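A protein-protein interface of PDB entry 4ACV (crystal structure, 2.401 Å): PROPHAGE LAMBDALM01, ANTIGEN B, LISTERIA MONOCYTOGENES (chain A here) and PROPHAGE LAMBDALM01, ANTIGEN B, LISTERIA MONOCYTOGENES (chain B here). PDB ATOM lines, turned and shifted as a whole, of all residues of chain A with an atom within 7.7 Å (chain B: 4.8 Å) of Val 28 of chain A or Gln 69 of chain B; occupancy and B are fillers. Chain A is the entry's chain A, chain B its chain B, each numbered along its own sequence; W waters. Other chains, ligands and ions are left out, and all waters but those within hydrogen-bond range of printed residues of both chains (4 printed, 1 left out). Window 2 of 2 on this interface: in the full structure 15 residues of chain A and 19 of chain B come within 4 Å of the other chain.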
ATOM      1  N   MET A   7      -8.988 -13.853  25.543  1.00  0.00           N
ATOM      2  CA  MET A   7      -8.124 -12.687  25.481  1.00  0.00           C
ATOM      3  C   MET A   7      -6.739 -13.029  24.929  1.00  0.00           C
ATOM      4  O   MET A   7      -6.151 -12.267  24.169  1.00  0.00           O
ATOM      5  CB  MET A   7      -8.022 -12.052  26.860  1.00  0.00           C
ATOM      6  CG  MET A   7      -7.888 -10.560  26.801  1.00  0.00           C
ATOM      7  SD  MET A   7      -7.993  -9.822  28.424  1.00  0.00           S
ATOM      8  CE  MET A   7      -6.998  -8.356  28.148  1.00  0.00           C
ATOM      9  N   LEU A  10      -7.311 -13.218  21.260  1.00  0.00           N
ATOM     10  CA  LEU A  10      -7.351 -11.841  20.766  1.00  0.00           C
ATOM     11  C   LEU A  10      -5.934 -11.287  20.597  1.00  0.00           C
ATOM     12  O   LEU A  10      -5.596 -10.731  19.561  1.00  0.00           O
ATOM     13  CB  LEU A  10      -8.153 -10.940  21.714  1.00  0.00           C
ATOM     14  CG  LEU A  10      -9.670 -11.122  21.812  1.00  0.00           C
ATOM     15  CD1 LEU A  10     -10.252 -10.241  22.927  1.00  0.00           C
ATOM     16  CD2 LEU A  10     -10.370 -10.845  20.472  1.00  0.00           C
ATOM     17  N   GLU A  11      -5.096 -11.469  21.610  1.00  0.00           N
ATOM     18  CA  GLU A  11      -3.740 -10.930  21.582  1.00  0.00           C
ATOM     19  C   GLU A  11      -2.898 -11.522  20.441  1.00  0.00           C
ATOM     20  O   GLU A  11      -2.174 -10.809  19.749  1.00  0.00           O
ATOM     21  CB  GLU A  11      -3.063 -11.151  22.937  1.00  0.00           C
ATOM     22  CG  GLU A  11      -1.875 -10.247  23.190  1.00  0.00           C
ATOM     23  CD  GLU A  11      -2.192  -8.786  22.911  1.00  0.00           C
ATOM     24  OE1 GLU A  11      -3.031  -8.214  23.642  1.00  0.00           O
ATOM     25  OE2 GLU A  11      -1.604  -8.219  21.957  1.00  0.00           O
ATOM     26  N   ARG A  14      -4.037  -9.952  17.145  1.00  0.00           N
ATOM     27  CA  ARG A  14      -3.525  -8.585  17.083  1.00  0.00           C
ATOM     28  C   ARG A  14      -2.038  -8.557  16.744  1.00  0.00           C
ATOM     29  O   ARG A  14      -1.607  -7.792  15.884  1.00  0.00           O
ATOM     30  CB  ARG A  14      -3.777  -7.848  18.397  1.00  0.00           C
ATOM     31  CG  ARG A  14      -2.904  -6.624  18.591  1.00  0.00           C
ATOM     32  CD  ARG A  14      -2.957  -6.117  20.016  1.00  0.00           C
ATOM     33  NE  ARG A  14      -3.361  -4.717  20.054  1.00  0.00           N
ATOM     34  CZ  ARG A  14      -2.511  -3.694  20.055  1.00  0.00           C
ATOM     35  NH1 ARG A  14      -1.204  -3.921  20.037  1.00  0.00           N
ATOM     36  NH2 ARG A  14      -2.965  -2.444  20.081  1.00  0.00           N
ATOM     37  N   VAL A  25      -4.168  -2.833  15.270  1.00  0.00           N
ATOM     38  CA  VAL A  25      -5.500  -3.335  15.611  1.00  0.00           C
ATOM     39  C   VAL A  25      -5.692  -3.377  17.119  1.00  0.00           C
ATOM     40  O   VAL A  25      -4.800  -3.786  17.853  1.00  0.00           O
ATOM     41  CB  VAL A  25      -5.770  -4.735  14.992  1.00  0.00           C
ATOM     42  CG1 VAL A  25      -7.232  -5.169  15.200  1.00  0.00           C
ATOM     43  CG2 VAL A  25      -5.442  -4.731  13.507  1.00  0.00           C
ATOM     44  N   SER A  26      -6.859  -2.935  17.571  1.00  0.00           N
ATOM     45  CA  SER A  26      -7.182  -2.919  18.993  1.00  0.00           C
ATOM     46  C   SER A  26      -8.045  -4.135  19.323  1.00  0.00           C
ATOM     47  O   SER A  26      -8.881  -4.544  18.518  1.00  0.00           O
ATOM     48  CB  SER A  26      -7.911  -1.624  19.353  1.00  0.00           C
ATOM     49  OG  SER A  26      -8.200  -1.566  20.732  1.00  0.00           O
ATOM     50  N   ILE A  27      -7.845  -4.724  20.497  1.00  0.00           N
ATOM     51  CA  ILE A  27      -8.590  -5.931  20.862  1.00  0.00           C
ATOM     52  C   ILE A  27      -9.821  -5.627  21.723  1.00  0.00           C
ATOM     53  O   ILE A  27     -10.514  -6.534  22.175  1.00  0.00           O
ATOM     54  CB  ILE A  27      -7.683  -6.993  21.556  1.00  0.00           C
ATOM     55  CG1 ILE A  27      -7.135  -6.459  22.879  1.00  0.00           C
ATOM     56  CG2 ILE A  27      -6.546  -7.379  20.643  1.00  0.00           C
ATOM     57  CD1 ILE A  27      -6.603  -7.532  23.793  1.00  0.00           C
ATOM     58  N   VAL A  28     -10.080  -4.342  21.938  1.00  0.00           N
ATOM     59  CA  VAL A  28     -11.207  -3.894  22.741  1.00  0.00           C
ATOM     60  C   VAL A  28     -12.333  -3.342  21.857  1.00  0.00           C
ATOM     61  O   VAL A  28     -12.139  -2.430  21.061  1.00  0.00           O
ATOM     62  CB  VAL A  28     -10.776  -2.816  23.765  1.00  0.00           C
ATOM     63  CG1 VAL A  28     -11.976  -2.239  24.472  1.00  0.00           C
ATOM     64  CG2 VAL A  28      -9.795  -3.401  24.772  1.00  0.00           C
ATOM     65  N   MET A  29     -13.510  -3.920  22.002  1.00  0.00           N
ATOM     66  CA  MET A  29     -14.673  -3.475  21.278  1.00  0.00           C
ATOM     67  C   MET A  29     -15.191  -2.165  21.876  1.00  0.00           C
ATOM     68  O   MET A  29     -15.299  -2.025  23.095  1.00  0.00           O
ATOM     69  CB  MET A  29     -15.753  -4.557  21.338  1.00  0.00           C
ATOM     70  CG  MET A  29     -16.957  -4.258  20.478  1.00  0.00           C
ATOM     71  SD  MET A  29     -16.506  -4.005  18.753  1.00  0.00           S
ATOM     72  CE  MET A  29     -18.109  -3.590  18.059  1.00  0.00           C
ATOM     73  N   ARG A  30     -15.497  -1.207  21.008  1.00  0.00           N
ATOM     74  CA  ARG A  30     -16.080   0.064  21.424  1.00  0.00           C
ATOM     75  C   ARG A  30     -17.314   0.309  20.569  1.00  0.00           C
ATOM     76  O   ARG A  30     -17.337  -0.048  19.394  1.00  0.00           O
ATOM     77  CB  ARG A  30     -15.073   1.211  21.271  1.00  0.00           C
ATOM     78  N   ASN A  31     -18.346   0.894  21.166  1.00  0.00           N
ATOM     79  CA  ASN A  31     -19.597   1.142  20.460  1.00  0.00           C
ATOM     80  C   ASN A  31     -19.512   2.355  19.540  1.00  0.00           C
ATOM     81  O   ASN A  31     -19.720   2.237  18.335  1.00  0.00           O
ATOM     82  CB  ASN A  31     -20.749   1.316  21.453  1.00  0.00           C
ATOM     83  N   THR A  37     -10.368   3.022  12.092  1.00  0.00           N
ATOM     84  CA  THR A  37      -9.830   2.099  13.075  1.00  0.00           C
ATOM     85  C   THR A  37     -10.182   0.643  12.752  1.00  0.00           C
ATOM     86  O   THR A  37     -11.110   0.347  11.994  1.00  0.00           O
ATOM     87  CB  THR A  37     -10.339   2.426  14.495  1.00  0.00           C
ATOM     88  OG1 THR A  37      -9.531   1.743  15.460  1.00  0.00           O
ATOM     89  CG2 THR A  37     -11.785   1.994  14.658  1.00  0.00           C
ATOM     90  N   THR A  38      -9.412  -0.259  13.343  1.00  0.00           N
ATOM     91  CA  THR A  38      -9.667  -1.682  13.249  1.00  0.00           C
ATOM     92  C   THR A  38      -9.649  -2.278  14.661  1.00  0.00           C
ATOM     93  O   THR A  38      -8.655  -2.157  15.394  1.00  0.00           O
ATOM     94  CB  THR A  38      -8.620  -2.363  12.360  1.00  0.00           C
ATOM     95  OG1 THR A  38      -8.364  -1.539  11.213  1.00  0.00           O
ATOM     96  CG2 THR A  38      -9.103  -3.745  11.917  1.00  0.00           C
ATOM     97  N   MET A  39     -10.768  -2.882  15.045  1.00  0.00           N
ATOM     98  CA  MET A  39     -10.885  -3.538  16.338  1.00  0.00           C
ATOM     99  C   MET A  39     -11.312  -4.980  16.138  1.00  0.00           C
ATOM    100  O   MET A  39     -12.000  -5.313  15.169  1.00  0.00           O
ATOM    101  CB  MET A  39     -11.928  -2.867  17.231  1.00  0.00           C
ATOM    102  CG  MET A  39     -11.985  -1.371  17.176  1.00  0.00           C
ATOM    103  SD  MET A  39     -13.449  -0.789  18.047  1.00  0.00           S
ATOM    104  CE  MET A  39     -14.732  -1.063  16.841  1.00  0.00           C
ATOM    105  N   ILE A  40     -10.906  -5.825  17.075  1.00  0.00           N
ATOM    106  CA  ILE A  40     -11.374  -7.187  17.119  1.00  0.00           C
ATOM    107  C   ILE A  40     -12.442  -7.316  18.203  1.00  0.00           C
ATOM    108  O   ILE A  40     -12.271  -6.833  19.324  1.00  0.00           O
ATOM    109  CB  ILE A  40     -10.214  -8.157  17.401  1.00  0.00           C
ATOM    110  CG1 ILE A  40      -9.067  -7.894  16.419  1.00  0.00           C
ATOM    111  CG2 ILE A  40     -10.710  -9.606  17.334  1.00  0.00           C
ATOM    112  CD1 ILE A  40      -7.782  -8.688  16.703  1.00  0.00           C
ATOM    113  N   GLU A  41     -13.552  -7.953  17.864  1.00  0.00           N
ATOM    114  CA  GLU A  41     -14.590  -8.175  18.850  1.00  0.00           C
ATOM    115  C   GLU A  41     -14.813  -9.662  19.099  1.00  0.00           C
ATOM    116  O   GLU A  41     -15.319 -10.382  18.237  1.00  0.00           O
ATOM    117  CB  GLU A  41     -15.888  -7.520  18.414  1.00  0.00           C
ATOM    118  CG  GLU A  41     -17.041  -7.764  19.368  1.00  0.00           C
ATOM    119  CD  GLU A  41     -18.383  -7.645  18.681  1.00  0.00           C
ATOM    120  OE1 GLU A  41     -18.409  -7.479  17.445  1.00  0.00           O
ATOM    121  OE2 GLU A  41     -19.414  -7.728  19.368  1.00  0.00           O
ATOM    122  N   MET A  42     -14.429 -10.120  20.281  1.00  0.00           N
ATOM    123  CA  MET A  42     -14.631 -11.513  20.635  1.00  0.00           C
ATOM    124  C   MET A  42     -16.125 -11.693  20.859  1.00  0.00           C
ATOM    125  O   MET A  42     -16.797 -10.794  21.365  1.00  0.00           O
ATOM    126  CB  MET A  42     -13.812 -11.881  21.885  1.00  0.00           C
ATOM    127  CG  MET A  42     -13.848 -13.358  22.282  1.00  0.00           C
ATOM    128  SD  MET A  42     -13.240 -14.557  21.053  1.00  0.00           S
ATOM    129  CE  MET A  42     -11.554 -14.023  20.822  1.00  0.00           C
ATOM    130  N   HIS A  63     -13.777  -5.531  13.003  1.00  0.00           N
ATOM    131  CA  HIS A  63     -14.420  -4.299  12.584  1.00  0.00           C
ATOM    132  C   HIS A  63     -13.401  -3.350  11.961  1.00  0.00           C
ATOM    133  O   HIS A  63     -12.414  -2.982  12.584  1.00  0.00           O
ATOM    134  CB  HIS A  63     -15.103  -3.624  13.762  1.00  0.00           C
ATOM    135  CG  HIS A  63     -16.157  -4.463  14.409  1.00  0.00           C
ATOM    136  ND1 HIS A  63     -17.488  -4.383  14.062  1.00  0.00           N
ATOM    137  CD2 HIS A  63     -16.077  -5.394  15.388  1.00  0.00           C
ATOM    138  CE1 HIS A  63     -18.183  -5.226  14.804  1.00  0.00           C
ATOM    139  NE2 HIS A  63     -17.350  -5.853  15.613  1.00  0.00           N
ATOM    140  N   THR B  66     -11.760  -3.274  34.829  1.00  0.00           N
ATOM    141  CA  THR B  66     -10.500  -2.663  35.213  1.00  0.00           C
ATOM    142  C   THR B  66     -10.359  -1.318  34.519  1.00  0.00           C
ATOM    143  O   THR B  66     -11.021  -1.059  33.514  1.00  0.00           O
ATOM    144  CB  THR B  66      -9.327  -3.545  34.795  1.00  0.00           C
ATOM    145  OG1 THR B  66      -9.541  -3.985  33.451  1.00  0.00           O
ATOM    146  CG2 THR B  66      -9.231  -4.754  35.698  1.00  0.00           C
ATOM    147  N   GLU B  68      -8.017  -0.405  32.746  1.00  0.00           N
ATOM    148  CA  GLU B  68      -7.432  -0.644  31.433  1.00  0.00           C
ATOM    149  C   GLU B  68      -7.215  -2.141  31.207  1.00  0.00           C
ATOM    150  O   GLU B  68      -7.468  -2.944  32.096  1.00  0.00           O
ATOM    151  CB  GLU B  68      -6.114   0.109  31.303  1.00  0.00           C
ATOM    152  CG  GLU B  68      -5.025  -0.430  32.179  1.00  0.00           C
ATOM    153  CD  GLU B  68      -3.809   0.462  32.161  1.00  0.00           C
ATOM    154  OE1 GLU B  68      -3.976   1.681  31.950  1.00  0.00           O
ATOM    155  OE2 GLU B  68      -2.688  -0.055  32.352  1.00  0.00           O
ATOM    156  N   GLN B  69      -6.756  -2.512  30.014  1.00  0.00           N
ATOM    157  CA  GLN B  69      -6.516  -3.914  29.699  1.00  0.00           C
ATOM    158  C   GLN B  69      -5.745  -4.626  30.802  1.00  0.00           C
ATOM    159  O   GLN B  69      -4.752  -4.119  31.315  1.00  0.00           O
ATOM    160  CB  GLN B  69      -5.795  -4.068  28.360  1.00  0.00           C
ATOM    161  CG  GLN B  69      -6.705  -3.940  27.159  1.00  0.00           C
ATOM    162  CD  GLN B  69      -5.955  -3.941  25.843  1.00  0.00           C
ATOM    163  OE1 GLN B  69      -6.121  -3.035  25.028  1.00  0.00           O
ATOM    164  NE2 GLN B  69      -5.128  -4.953  25.626  1.00  0.00           N
ATOM    165  N   ASP B  70      -6.222  -5.809  31.162  1.00  0.00           N
ATOM    166  CA  ASP B  70      -5.630  -6.575  32.241  1.00  0.00           C
ATOM    167  C   ASP B  70      -5.642  -8.061  31.883  1.00  0.00           C
ATOM    168  O   ASP B  70      -6.406  -8.844  32.445  1.00  0.00           O
ATOM    169  CB  ASP B  70      -6.386  -6.309  33.548  1.00  0.00           C
ATOM    170  CG  ASP B  70      -5.842  -7.110  34.715  1.00  0.00           C
ATOM    171  OD1 ASP B  70      -4.708  -7.618  34.604  1.00  0.00           O
ATOM    172  OD2 ASP B  70      -6.546  -7.233  35.745  1.00  0.00           O
ATOM    173  N   LEU B  71      -4.800  -8.436  30.926  1.00  0.00           N
ATOM    174  CA  LEU B  71      -4.698  -9.828  30.491  1.00  0.00           C
ATOM    175  C   LEU B  71      -4.153 -10.731  31.593  1.00  0.00           C
ATOM    176  O   LEU B  71      -4.592 -11.877  31.740  1.00  0.00           O
ATOM    177  CB  LEU B  71      -3.807  -9.955  29.248  1.00  0.00           C
ATOM    178  CG  LEU B  71      -3.553 -11.407  28.804  1.00  0.00           C
ATOM    179  CD1 LEU B  71      -4.601 -11.859  27.806  1.00  0.00           C
ATOM    180  CD2 LEU B  71      -2.171 -11.562  28.205  1.00  0.00           C
ATOM    181  N   LEU B 104     -14.724  -8.492  25.409  1.00  0.00           N
ATOM    182  CA  LEU B 104     -13.795  -7.500  25.904  1.00  0.00           C
ATOM    183  C   LEU B 104     -14.272  -6.193  25.310  1.00  0.00           C
ATOM    184  O   LEU B 104     -14.112  -5.950  24.108  1.00  0.00           O
ATOM    185  CB  LEU B 104     -12.351  -7.811  25.475  1.00  0.00           C
ATOM    186  CG  LEU B 104     -11.298  -6.902  26.126  1.00  0.00           C
ATOM    187  CD1 LEU B 104     -11.392  -6.971  27.651  1.00  0.00           C
ATOM    188  CD2 LEU B 104      -9.883  -7.233  25.658  1.00  0.00           C
ATOM    189  N   VAL B 105     -14.882  -5.358  26.145  1.00  0.00           N
ATOM    190  CA  VAL B 105     -15.520  -4.153  25.643  1.00  0.00           C
ATOM    191  C   VAL B 105     -15.277  -2.942  26.551  1.00  0.00           C
ATOM    192  O   VAL B 105     -15.159  -3.075  27.765  1.00  0.00           O
ATOM    193  CB  VAL B 105     -17.042  -4.397  25.423  1.00  0.00           C
ATOM    194  CG1 VAL B 105     -17.714  -4.751  26.732  1.00  0.00           C
ATOM    195  CG2 VAL B 105     -17.707  -3.186  24.785  1.00  0.00           C
ATOM    196  N   LYS B 106     -15.190  -1.763  25.944  1.00  0.00           N
ATOM    197  CA  LYS B 106     -15.075  -0.515  26.688  1.00  0.00           C
ATOM    198  C   LYS B 106     -16.445  -0.035  27.175  1.00  0.00           C
ATOM    199  O   LYS B 106     -17.401   0.031  26.398  1.00  0.00           O
ATOM    200  CB  LYS B 106     -14.421   0.562  25.819  1.00  0.00           C
ATOM    201  CG  LYS B 106     -14.550   1.992  26.361  1.00  0.00           C
ATOM    202  CD  LYS B 106     -13.785   2.977  25.473  1.00  0.00           C
ATOM    203  CE  LYS B 106     -13.843   4.407  26.006  1.00  0.00           C
ATOM    204  NZ  LYS B 106     -15.253   4.841  26.169  1.00  0.00           N
ATOM    205  N   ILE B 111     -12.570  -0.966  31.179  1.00  0.00           N
ATOM    206  CA  ILE B 111     -12.488  -2.127  30.306  1.00  0.00           C
ATOM    207  C   ILE B 111     -13.273  -3.296  30.940  1.00  0.00           C
ATOM    208  O   ILE B 111     -12.995  -3.744  32.056  1.00  0.00           O
ATOM    209  CB  ILE B 111     -11.022  -2.519  30.038  1.00  0.00           C
ATOM    210  CG1 ILE B 111     -10.265  -1.340  29.399  1.00  0.00           C
ATOM    211  CG2 ILE B 111     -10.945  -3.768  29.170  1.00  0.00           C
ATOM    212  CD1 ILE B 111     -10.883  -0.828  28.107  1.00  0.00           C
HETATM  213  O   HOH W   1     -16.026  -8.325  22.734  1.00  0.00           O
HETATM  214  O   HOH W   2      -3.703  -5.471  23.349  1.00  0.00           O
HETATM  215  O   HOH W   3      -5.407  -3.353  22.089  1.00  0.00           O
HETATM  216  O   HOH W   4      -8.873  -6.913  30.632  1.00  0.00           O
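Printed residues of chain B within 4 Å of Val 28 of chain A: Gln 69 (3.7 Å), Leu 104 (3.8 Å), Val 105 (3.96 Å) and Lys 106 (3.6 Å). Gln 69 of chain B touches just these residues of chain A: Ile 27 (3.5 Å) and Val 28 (3.7 Å). Of the printed residues of chain A, Lys 106 of chain B touches Val 28 (3.6 Å) and Met 29 (2.9 Å). Of the printed residues of chain B, Ile 27 of chain A touches Gln 69 and Leu 104. The nearest residue of chain B that does not touch Val 28 of chain A is Ile 111 of chain B (4.05 Å). The nearest residue of chain A that does not touch Gln 69 of chain B is Glu 11 of chain A (4.4 Å). The nearest printed residue of chain A that does not touch Val 105 of chain B is Arg 30 of chain A (4.8 Å).
N of Met 29 of chain A sits at hydrogen-bond distance from O of Leu 104 of chain B (3.0 Å). The backbone NH (N) of Lys 106 of chain B lies within hydrogen-bond range of the backbone carbonyl oxygen (O) of Met 29 of chain A, 2.9 Å away.
Met 7 of chain A touches Asp 70 of chain B (CE to C, 3.98 Å). Leu 71 of chain B touches Met 7 of chain A (N to CE, 3.5 Å). CE of Met 7 of chain A touches CD2 of Leu 104 of chain B (3.97 Å). Gln 69 of chain B touches Ile 27 of chain A (NE2 to CD1, 3.5 Å). O of Ile 27 of chain A touches CD2 of Leu 104 of chain B, 3.6 Å away. Val 28 of chain A touches Gln 69 of chain B. CA of Val 28 of chain A touches O of Leu 104 of chain B, at 3.8 Å. Val 105 of chain B touches Val 28 of chain A (C to CG1, 3.96 Å). CG1 of Val 28 of chain A touches N of Lys 106 of chain B (3.6 Å). Val 105 of chain B touches Met 29 of chain A.
Of the 18 printed residues of chain A, 4 touch a printed residue of chain B. Hydrophobic or aromatic side chains of chain A that line the printed part of chain B: Met 7, Ile 27, Val 28 and Met 29. Printed residues of chain B that touch a printed residue of chain A: Gln 69, Asp 70, Leu 71, Leu 104, Val 105 and Lys 106.
The side-chain sulfur (SD) of Met 29 of chain A lies close to a ring nitrogen (NE2) of His 63 of chain A, at 3.7 Å.
Water W2 lies within hydrogen-bond range of NE2 of Gln 69 of chain B, OE1 of Glu 11 of chain A and NE of Arg 14 of chain A. Water W4 bridges the backbone NH (N) of Asp 70 of chain B (2.9 Å) and the side-chain sulfur (SD) of Met 7 of chain A (3.8 Å). Water W1 lies within hydrogen-bond range of O of Met 42 of chain A (2.9 Å) and N of Leu 104 of chain B (3.0 Å). Water W3 lies within hydrogen-bond range of the side-chain amide oxygen (OE1) of Gln 69 of chain B (3.0 Å), the guanidinium group (NE) of Arg 14 of chain A (3.2 Å) and the backbone NH (N) of Ile 27 of chain A (3.2 Å).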
